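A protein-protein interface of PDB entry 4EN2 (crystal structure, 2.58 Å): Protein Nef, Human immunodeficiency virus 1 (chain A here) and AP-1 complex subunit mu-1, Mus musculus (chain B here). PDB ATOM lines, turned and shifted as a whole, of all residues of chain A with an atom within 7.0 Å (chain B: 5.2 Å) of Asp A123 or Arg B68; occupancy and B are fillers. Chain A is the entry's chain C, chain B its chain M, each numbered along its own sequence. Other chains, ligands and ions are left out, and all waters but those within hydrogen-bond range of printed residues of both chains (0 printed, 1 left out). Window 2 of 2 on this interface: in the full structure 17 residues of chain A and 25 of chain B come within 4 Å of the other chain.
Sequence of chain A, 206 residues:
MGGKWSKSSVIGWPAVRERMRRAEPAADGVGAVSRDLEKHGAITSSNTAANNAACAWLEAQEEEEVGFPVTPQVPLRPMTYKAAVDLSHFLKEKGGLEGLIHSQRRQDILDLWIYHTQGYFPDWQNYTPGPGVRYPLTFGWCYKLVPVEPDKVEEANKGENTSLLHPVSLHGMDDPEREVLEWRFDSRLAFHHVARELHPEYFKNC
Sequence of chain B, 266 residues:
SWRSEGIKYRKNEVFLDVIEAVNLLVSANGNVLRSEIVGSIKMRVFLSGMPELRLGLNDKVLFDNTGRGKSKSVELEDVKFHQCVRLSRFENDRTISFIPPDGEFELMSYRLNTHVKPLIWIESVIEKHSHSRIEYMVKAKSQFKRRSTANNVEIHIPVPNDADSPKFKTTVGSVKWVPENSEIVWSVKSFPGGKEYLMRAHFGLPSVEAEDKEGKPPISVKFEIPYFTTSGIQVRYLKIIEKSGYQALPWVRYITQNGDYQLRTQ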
ATOM      1  N   ARG A  77       7.446   2.544 -14.642  1.00  0.00           N
ATOM      2  CA  ARG A  77       8.470   1.616 -14.212  1.00  0.00           C
ATOM      3  C   ARG A  77       7.961   0.211 -14.022  1.00  0.00           C
ATOM      4  O   ARG A  77       6.760  -0.021 -13.910  1.00  0.00           O
ATOM      5  CB  ARG A  77       9.151   2.104 -12.931  1.00  0.00           C
ATOM      6  CG  ARG A  77       8.267   2.065 -11.707  1.00  0.00           C
ATOM      7  CD  ARG A  77       7.403   3.298 -11.678  1.00  0.00           C
ATOM      8  NE  ARG A  77       6.610   3.317 -10.469  1.00  0.00           N
ATOM      9  CZ  ARG A  77       5.582   4.125 -10.256  1.00  0.00           C
ATOM     10  NH1 ARG A  77       5.209   4.991 -11.188  1.00  0.00           N
ATOM     11  NH2 ARG A  77       4.922   4.057  -9.107  1.00  0.00           N
ATOM     12  N   PRO A  78       8.900  -0.736 -14.008  1.00  0.00           N
ATOM     13  CA  PRO A  78       8.487  -2.083 -13.714  1.00  0.00           C
ATOM     14  C   PRO A  78       8.101  -2.214 -12.259  1.00  0.00           C
ATOM     15  O   PRO A  78       8.587  -1.478 -11.412  1.00  0.00           O
ATOM     16  CB  PRO A  78       9.739  -2.933 -14.026  1.00  0.00           C
ATOM     17  CG  PRO A  78      10.759  -2.005 -14.600  1.00  0.00           C
ATOM     18  CD  PRO A  78      10.360  -0.633 -14.186  1.00  0.00           C
ATOM     19  N   MET A  79       7.197  -3.141 -12.009  1.00  0.00           N
ATOM     20  CA  MET A  79       6.766  -3.492 -10.666  1.00  0.00           C
ATOM     21  C   MET A  79       7.952  -3.806  -9.773  1.00  0.00           C
ATOM     22  O   MET A  79       8.892  -4.499 -10.174  1.00  0.00           O
ATOM     23  CB  MET A  79       5.855  -4.722 -10.707  1.00  0.00           C
ATOM     24  CG  MET A  79       5.458  -5.285  -9.336  1.00  0.00           C
ATOM     25  SD  MET A  79       4.260  -4.245  -8.533  1.00  0.00           S
ATOM     26  CE  MET A  79       2.817  -4.641  -9.480  1.00  0.00           C
ATOM     27  N   ASP A 111      -3.856  -6.068 -14.501  1.00  0.00           N
ATOM     28  CA  ASP A 111      -2.597  -5.428 -14.886  1.00  0.00           C
ATOM     29  C   ASP A 111      -2.759  -4.005 -15.372  1.00  0.00           C
ATOM     30  O   ASP A 111      -1.912  -3.159 -15.101  1.00  0.00           O
ATOM     31  CB  ASP A 111      -1.912  -6.217 -15.990  1.00  0.00           C
ATOM     32  CG  ASP A 111      -1.440  -7.568 -15.519  1.00  0.00           C
ATOM     33  OD1 ASP A 111      -2.086  -8.074 -14.583  1.00  0.00           O
ATOM     34  OD2 ASP A 111      -0.450  -8.127 -16.068  1.00  0.00           O
ATOM     35  N   TYR A 120       2.896   1.145 -13.292  1.00  0.00           N
ATOM     36  CA  TYR A 120       3.678  -0.066 -13.484  1.00  0.00           C
ATOM     37  C   TYR A 120       3.369  -0.690 -14.817  1.00  0.00           C
ATOM     38  O   TYR A 120       2.231  -1.111 -15.078  1.00  0.00           O
ATOM     39  CB  TYR A 120       3.460  -1.103 -12.370  1.00  0.00           C
ATOM     40  CG  TYR A 120       3.982  -0.645 -11.044  1.00  0.00           C
ATOM     41  CD1 TYR A 120       5.346  -0.426 -10.851  1.00  0.00           C
ATOM     42  CD2 TYR A 120       3.111  -0.394  -9.992  1.00  0.00           C
ATOM     43  CE1 TYR A 120       5.812   0.021  -9.646  1.00  0.00           C
ATOM     44  CE2 TYR A 120       3.570   0.048  -8.782  1.00  0.00           C
ATOM     45  CZ  TYR A 120       4.912   0.253  -8.619  1.00  0.00           C
ATOM     46  OH  TYR A 120       5.336   0.682  -7.403  1.00  0.00           O
ATOM     47  N   PHE A 121       4.410  -0.765 -15.636  1.00  0.00           N
ATOM     48  CA  PHE A 121       4.322  -1.451 -16.904  1.00  0.00           C
ATOM     49  C   PHE A 121       3.658  -2.774 -16.628  1.00  0.00           C
ATOM     50  O   PHE A 121       4.080  -3.494 -15.734  1.00  0.00           O
ATOM     51  CB  PHE A 121       5.696  -1.739 -17.501  1.00  0.00           C
ATOM     52  CG  PHE A 121       6.481  -0.531 -17.811  1.00  0.00           C
ATOM     53  CD1 PHE A 121       7.723  -0.326 -17.240  1.00  0.00           C
ATOM     54  CD2 PHE A 121       5.983   0.416 -18.692  1.00  0.00           C
ATOM     55  CE1 PHE A 121       8.456   0.814 -17.533  1.00  0.00           C
ATOM     56  CE2 PHE A 121       6.710   1.554 -18.979  1.00  0.00           C
ATOM     57  CZ  PHE A 121       7.941   1.760 -18.394  1.00  0.00           C
ATOM     58  N   PRO A 122       2.618  -3.115 -17.401  1.00  0.00           N
ATOM     59  CA  PRO A 122       1.918  -4.381 -17.215  1.00  0.00           C
ATOM     60  C   PRO A 122       2.623  -5.543 -17.892  1.00  0.00           C
ATOM     61  O   PRO A 122       2.007  -6.307 -18.626  1.00  0.00           O
ATOM     62  CB  PRO A 122       0.577  -4.115 -17.865  1.00  0.00           C
ATOM     63  CG  PRO A 122       0.912  -3.186 -18.979  1.00  0.00           C
ATOM     64  CD  PRO A 122       2.016  -2.313 -18.477  1.00  0.00           C
ATOM     65  N   ASP A 123       3.912  -5.676 -17.632  1.00  0.00           N
ATOM     66  CA  ASP A 123       4.687  -6.863 -18.039  1.00  0.00           C
ATOM     67  C   ASP A 123       5.111  -7.710 -16.827  1.00  0.00           C
ATOM     68  O   ASP A 123       5.918  -8.635 -16.944  1.00  0.00           O
ATOM     69  CB  ASP A 123       5.933  -6.440 -18.835  1.00  0.00           C
ATOM     70  CG  ASP A 123       6.738  -5.349 -18.130  1.00  0.00           C
ATOM     71  OD1 ASP A 123       7.052  -5.508 -16.904  1.00  0.00           O
ATOM     72  OD2 ASP A 123       7.035  -4.318 -18.801  1.00  0.00           O
ATOM     73  N   TRP A 124       4.531  -7.434 -15.669  1.00  0.00           N
ATOM     74  CA  TRP A 124       4.989  -8.062 -14.417  1.00  0.00           C
ATOM     75  C   TRP A 124       4.252  -9.295 -13.992  1.00  0.00           C
ATOM     76  O   TRP A 124       4.795 -10.080 -13.238  1.00  0.00           O
ATOM     77  CB  TRP A 124       4.961  -7.047 -13.278  1.00  0.00           C
ATOM     78  CG  TRP A 124       3.586  -6.562 -12.996  1.00  0.00           C
ATOM     79  CD1 TRP A 124       2.950  -5.472 -13.537  1.00  0.00           C
ATOM     80  CD2 TRP A 124       2.639  -7.171 -12.109  1.00  0.00           C
ATOM     81  NE1 TRP A 124       1.689  -5.359 -13.028  1.00  0.00           N
ATOM     82  CE2 TRP A 124       1.443  -6.352 -12.170  1.00  0.00           C
ATOM     83  CE3 TRP A 124       2.660  -8.290 -11.304  1.00  0.00           C
ATOM     84  CZ2 TRP A 124       0.331  -6.653 -11.449  1.00  0.00           C
ATOM     85  CZ3 TRP A 124       1.542  -8.600 -10.575  1.00  0.00           C
ATOM     86  CH2 TRP A 124       0.399  -7.795 -10.632  1.00  0.00           C
ATOM     87  N   GLN A 125       2.996  -9.443 -14.362  1.00  0.00           N
ATOM     88  CA  GLN A 125       2.222 -10.580 -13.897  1.00  0.00           C
ATOM     89  C   GLN A 125       2.312 -11.790 -14.834  1.00  0.00           C
ATOM     90  O   GLN A 125       1.332 -12.439 -15.155  1.00  0.00           O
ATOM     91  CB  GLN A 125       0.771 -10.193 -13.659  1.00  0.00           C
ATOM     92  CG  GLN A 125       0.065 -11.198 -12.773  1.00  0.00           C
ATOM     93  CD  GLN A 125      -1.362 -10.839 -12.444  1.00  0.00           C
ATOM     94  OE1 GLN A 125      -2.160 -11.722 -12.097  1.00  0.00           O
ATOM     95  NE2 GLN A 125      -1.701  -9.555 -12.543  1.00  0.00           N
ATOM     96  N   ASN A 126       3.506 -12.153 -15.233  1.00  0.00           N
ATOM     97  CA  ASN A 126       3.649 -13.407 -15.923  1.00  0.00           C
ATOM     98  C   ASN A 126       3.995 -14.520 -14.944  1.00  0.00           C
ATOM     99  O   ASN A 126       4.600 -14.302 -13.887  1.00  0.00           O
ATOM    100  CB  ASN A 126       4.678 -13.296 -17.061  1.00  0.00           C
ATOM    101  CG  ASN A 126       4.216 -12.365 -18.153  1.00  0.00           C
ATOM    102  OD1 ASN A 126       3.224 -12.636 -18.825  1.00  0.00           O
ATOM    103  ND2 ASN A 126       4.898 -11.235 -18.315  1.00  0.00           N
ATOM    104  N   LEU A 137       6.765 -14.754 -12.092  1.00  0.00           N
ATOM    105  CA  LEU A 137       8.098 -14.327 -12.441  1.00  0.00           C
ATOM    106  C   LEU A 137       8.561 -13.147 -11.605  1.00  0.00           C
ATOM    107  O   LEU A 137       9.742 -12.979 -11.358  1.00  0.00           O
ATOM    108  CB  LEU A 137       8.158 -13.931 -13.908  1.00  0.00           C
ATOM    109  CG  LEU A 137       7.841 -15.018 -14.937  1.00  0.00           C
ATOM    110  CD1 LEU A 137       8.244 -14.502 -16.312  1.00  0.00           C
ATOM    111  CD2 LEU A 137       8.537 -16.341 -14.611  1.00  0.00           C
ATOM    112  N   THR A 138       7.624 -12.333 -11.167  1.00  0.00           N
ATOM    113  CA  THR A 138       7.965 -11.184 -10.331  1.00  0.00           C
ATOM    114  C   THR A 138       8.092 -11.563  -8.860  1.00  0.00           C
ATOM    115  O   THR A 138       7.111 -11.884  -8.213  1.00  0.00           O
ATOM    116  CB  THR A 138       6.958 -10.042 -10.504  1.00  0.00           C
ATOM    117  OG1 THR A 138       6.891  -9.689 -11.896  1.00  0.00           O
ATOM    118  CG2 THR A 138       7.379  -8.837  -9.677  1.00  0.00           C
ATOM    119  N   TYR A 202      15.233 -16.969 -17.539  1.00  0.00           N
ATOM    120  CA  TYR A 202      14.345 -15.830 -17.507  1.00  0.00           C
ATOM    121  C   TYR A 202      14.941 -14.679 -16.718  1.00  0.00           C
ATOM    122  O   TYR A 202      14.456 -13.555 -16.806  1.00  0.00           O
ATOM    123  CB  TYR A 202      13.036 -16.203 -16.840  1.00  0.00           C
ATOM    124  CG  TYR A 202      12.180 -17.169 -17.611  1.00  0.00           C
ATOM    125  CD1 TYR A 202      12.625 -17.779 -18.790  1.00  0.00           C
ATOM    126  CD2 TYR A 202      10.927 -17.511 -17.142  1.00  0.00           C
ATOM    127  CE1 TYR A 202      11.830 -18.665 -19.473  1.00  0.00           C
ATOM    128  CE2 TYR A 202      10.120 -18.402 -17.835  1.00  0.00           C
ATOM    129  CZ  TYR A 202      10.580 -18.973 -18.997  1.00  0.00           C
ATOM    130  OH  TYR A 202       9.777 -19.874 -19.659  1.00  0.00           O
ATOM    131  N   LEU B  62      13.599 -10.582 -26.157  1.00  0.00           N
ATOM    132  CA  LEU B  62      13.910 -10.673 -24.727  1.00  0.00           C
ATOM    133  C   LEU B  62      12.709 -11.147 -23.945  1.00  0.00           C
ATOM    134  O   LEU B  62      12.828 -11.971 -23.044  1.00  0.00           O
ATOM    135  CB  LEU B  62      14.349  -9.308 -24.176  1.00  0.00           C
ATOM    136  CG  LEU B  62      14.383  -9.083 -22.656  1.00  0.00           C
ATOM    137  CD1 LEU B  62      15.589  -9.750 -21.982  1.00  0.00           C
ATOM    138  CD2 LEU B  62      14.400  -7.604 -22.366  1.00  0.00           C
ATOM    139  N   PHE B  63      11.556 -10.594 -24.260  1.00  0.00           N
ATOM    140  CA  PHE B  63      10.357 -10.967 -23.549  1.00  0.00           C
ATOM    141  C   PHE B  63      10.042 -12.396 -23.845  1.00  0.00           C
ATOM    142  O   PHE B  63       9.848 -13.189 -22.925  1.00  0.00           O
ATOM    143  CB  PHE B  63       9.192 -10.059 -23.945  1.00  0.00           C
ATOM    144  CG  PHE B  63       9.122  -8.791 -23.155  1.00  0.00           C
ATOM    145  CD1 PHE B  63      10.224  -8.316 -22.469  1.00  0.00           C
ATOM    146  CD2 PHE B  63       7.938  -8.088 -23.088  1.00  0.00           C
ATOM    147  CE1 PHE B  63      10.126  -7.152 -21.710  1.00  0.00           C
ATOM    148  CE2 PHE B  63       7.841  -6.922 -22.346  1.00  0.00           C
ATOM    149  CZ  PHE B  63       8.931  -6.454 -21.648  1.00  0.00           C
ATOM    150  N   ASP B  64      10.037 -12.735 -25.134  1.00  0.00           N
ATOM    151  CA  ASP B  64       9.815 -14.131 -25.553  1.00  0.00           C
ATOM    152  C   ASP B  64      10.752 -15.108 -24.812  1.00  0.00           C
ATOM    153  O   ASP B  64      10.331 -16.138 -24.324  1.00  0.00           O
ATOM    154  CB  ASP B  64       9.983 -14.288 -27.058  1.00  0.00           C
ATOM    155  CG  ASP B  64       8.797 -13.728 -27.849  1.00  0.00           C
ATOM    156  OD1 ASP B  64       7.727 -13.492 -27.255  1.00  0.00           O
ATOM    157  OD2 ASP B  64       8.924 -13.525 -29.080  1.00  0.00           O
ATOM    158  N   THR B  66      12.224 -14.586 -21.864  1.00  0.00           N
ATOM    159  CA  THR B  66      12.203 -14.496 -20.417  1.00  0.00           C
ATOM    160  C   THR B  66      10.812 -14.726 -19.892  1.00  0.00           C
ATOM    161  O   THR B  66      10.443 -14.238 -18.839  1.00  0.00           O
ATOM    162  CB  THR B  66      12.759 -13.169 -19.921  1.00  0.00           C
ATOM    163  OG1 THR B  66      11.978 -12.080 -20.441  1.00  0.00           O
ATOM    164  CG2 THR B  66      14.184 -13.030 -20.330  1.00  0.00           C
ATOM    165  N   GLY B  67      10.036 -15.492 -20.636  1.00  0.00           N
ATOM    166  CA  GLY B  67       8.708 -15.909 -20.199  1.00  0.00           C
ATOM    167  C   GLY B  67       7.673 -14.791 -20.245  1.00  0.00           C
ATOM    168  O   GLY B  67       6.602 -14.878 -19.644  1.00  0.00           O
ATOM    169  N   ARG B  68       7.990 -13.729 -20.966  1.00  0.00           N
ATOM    170  CA  ARG B  68       7.136 -12.558 -20.987  1.00  0.00           C
ATOM    171  C   ARG B  68       6.546 -12.274 -22.350  1.00  0.00           C
ATOM    172  O   ARG B  68       6.077 -11.181 -22.614  1.00  0.00           O
ATOM    173  CB  ARG B  68       7.919 -11.365 -20.483  1.00  0.00           C
ATOM    174  CG  ARG B  68       8.223 -11.509 -19.009  1.00  0.00           C
ATOM    175  CD  ARG B  68       8.993 -10.333 -18.497  1.00  0.00           C
ATOM    176  NE  ARG B  68      10.366 -10.379 -18.963  1.00  0.00           N
ATOM    177  CZ  ARG B  68      11.294  -9.507 -18.591  1.00  0.00           C
ATOM    178  NH1 ARG B  68      10.982  -8.540 -17.734  1.00  0.00           N
ATOM    179  NH2 ARG B  68      12.527  -9.612 -19.060  1.00  0.00           N
ATOM    180  N   GLY B  69       6.522 -13.297 -23.193  1.00  0.00           N
ATOM    181  CA  GLY B  69       5.971 -13.217 -24.538  1.00  0.00           C
ATOM    182  C   GLY B  69       4.533 -12.783 -24.597  1.00  0.00           C
ATOM    183  O   GLY B  69       4.125 -12.146 -25.552  1.00  0.00           O
ATOM    184  N   LYS B  70       3.763 -13.112 -23.573  1.00  0.00           N
ATOM    185  CA  LYS B  70       2.358 -12.707 -23.513  1.00  0.00           C
ATOM    186  C   LYS B  70       2.221 -11.193 -23.427  1.00  0.00           C
ATOM    187  O   LYS B  70       1.160 -10.653 -23.679  1.00  0.00           O
ATOM    188  CB  LYS B  70       1.663 -13.326 -22.296  1.00  0.00           C
ATOM    189  CG  LYS B  70       0.688 -14.457 -22.603  1.00  0.00           C
ATOM    190  CD  LYS B  70       1.352 -15.566 -23.403  1.00  0.00           C
ATOM    191  CE  LYS B  70       0.836 -16.953 -23.066  1.00  0.00           C
ATOM    192  NZ  LYS B  70       1.495 -17.947 -23.964  1.00  0.00           N
ATOM    193  N   SER B  71       3.303 -10.526 -23.045  1.00  0.00           N
ATOM    194  CA  SER B  71       3.330  -9.087 -22.895  1.00  0.00           C
ATOM    195  C   SER B  71       3.678  -8.337 -24.177  1.00  0.00           C
ATOM    196  O   SER B  71       4.382  -8.851 -25.037  1.00  0.00           O
ATOM    197  CB  SER B  71       4.322  -8.669 -21.791  1.00  0.00           C
ATOM    198  OG  SER B  71       3.785  -8.903 -20.507  1.00  0.00           O
ATOM    199  N   GLN B 234       9.673   1.238 -25.467  1.00  0.00           N
ATOM    200  CA  GLN B 234       9.765   1.821 -24.127  1.00  0.00           C
ATOM    201  C   GLN B 234      11.075   1.417 -23.468  1.00  0.00           C
ATOM    202  O   GLN B 234      11.543   0.282 -23.607  1.00  0.00           O
ATOM    203  CB  GLN B 234       8.576   1.447 -23.229  1.00  0.00           C
ATOM    204  CG  GLN B 234       8.185  -0.017 -23.273  1.00  0.00           C
ATOM    205  CD  GLN B 234       7.185  -0.414 -22.177  1.00  0.00           C
ATOM    206  OE1 GLN B 234       6.301   0.370 -21.812  1.00  0.00           O
ATOM    207  NE2 GLN B 234       7.327  -1.636 -21.641  1.00  0.00           N
ATOM    208  N   ARG B 236      12.249   0.493 -20.240  1.00  0.00           N
ATOM    209  CA  ARG B 236      11.687   0.013 -19.002  1.00  0.00           C
ATOM    210  C   ARG B 236      12.493   0.489 -17.812  1.00  0.00           C
ATOM    211  O   ARG B 236      11.956   0.978 -16.796  1.00  0.00           O
ATOM    212  CB  ARG B 236      11.642  -1.498 -19.061  1.00  0.00           C
ATOM    213  CG  ARG B 236      10.740  -1.942 -20.191  1.00  0.00           C
ATOM    214  CD  ARG B 236      10.506  -3.426 -20.191  1.00  0.00           C
ATOM    215  NE  ARG B 236       9.847  -3.893 -18.956  1.00  0.00           N
ATOM    216  CZ  ARG B 236      10.444  -4.556 -17.958  1.00  0.00           C
ATOM    217  NH1 ARG B 236      11.732  -4.874 -18.022  1.00  0.00           N
ATOM    218  NH2 ARG B 236       9.749  -4.909 -16.889  1.00  0.00           N
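The side-chain hydroxyl of Ser B71 lies within hydrogen-bond range of the side-chain amide nitrogen of Asn A126.
The guanidinium group of Arg B236 is in salt-bridge range of the side-chain carboxylate of Asp A123 (2.8 Å).
OG1 of Thr B66 sits at hydrogen-bond distance from NE of Arg B68.
O of Phe B63 lies within hydrogen-bond range of OG1 of Thr B66 (3.5 Å).
The backbone carbonyl oxygen of Leu B62 sits at hydrogen-bond distance from the side-chain hydroxyl of Thr B66 (2.7 Å).
O of Asn A126 sits at hydrogen-bond distance from N of Leu A137 (2.8 Å).
The backbone carbonyl oxygen of Arg A77 sits at hydrogen-bond distance from the backbone NH of Phe A121, at 3.0 Å.
The backbone carbonyl oxygen of Asp A123 is in hydrogen-bond range of the side-chain amide nitrogen of Asn A126 (3.1 Å).
Among the printed residues, merely in contact across the chains: Pro A78 with Arg B236 (3.5 Å), Phe A121 with Gln B234 (3.1 Å), Phe A121 with Arg B236 (3.6 Å), Pro A122 with Ser B71 (3.7 Å), Asp A123 with Arg B68 (3.8 Å), Asp A123 with Ser B71 (3.3 Å), Asp A123 with Gln B234 (3.9 Å), Asn A126 with Gly B67 (3.6 Å), Asn A126 with Arg B68 (3.4 Å), Asn A126 with Lys B70 (3.9 Å), Leu A137 with Thr B66 (3.4 Å), Leu A137 with Gly B67 (3.7 Å), Tyr A202 with Thr B66 (3.6 Å) and Tyr A202 with Gly B67 (3.7 Å).
Of chain B, only Arg B68, Ser B71, Gln B234 and Arg B236 come within 4 Å of Asp A123.
Arg B68 touches just these residues of chain A: Asp A123 (3.8 Å) and Asn A126 (3.4 Å).
Gly B67 touches three residues of chain A.
Of the printed residues of chain B, Pro A78 touches Arg B236.
Printed residues of chain B within 4 Å of Asn A126: Gly B67 (3.6 Å), Arg B68 (3.4 Å), Lys B70 (3.9 Å) and Ser B71 (3.4 Å).
Of the printed residues of chain A, Arg B236 touches Pro A78, Phe A121 and Asp A123.
Tyr A120 touches none of the printed residues of chain B.
Phe B63 touches none of the printed residues of chain A.
Of the 11 printed residues of chain B, 7 touch a printed residue of chain A.
Along chain A the printed residues that touch a printed residue of chain B span positions 78 to 202.
Among the printed residues, Asp or Glu carboxylates within 4 Å of a Lys or Arg side-chain nitrogen of the other chain: Asp A123 with Arg B236.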
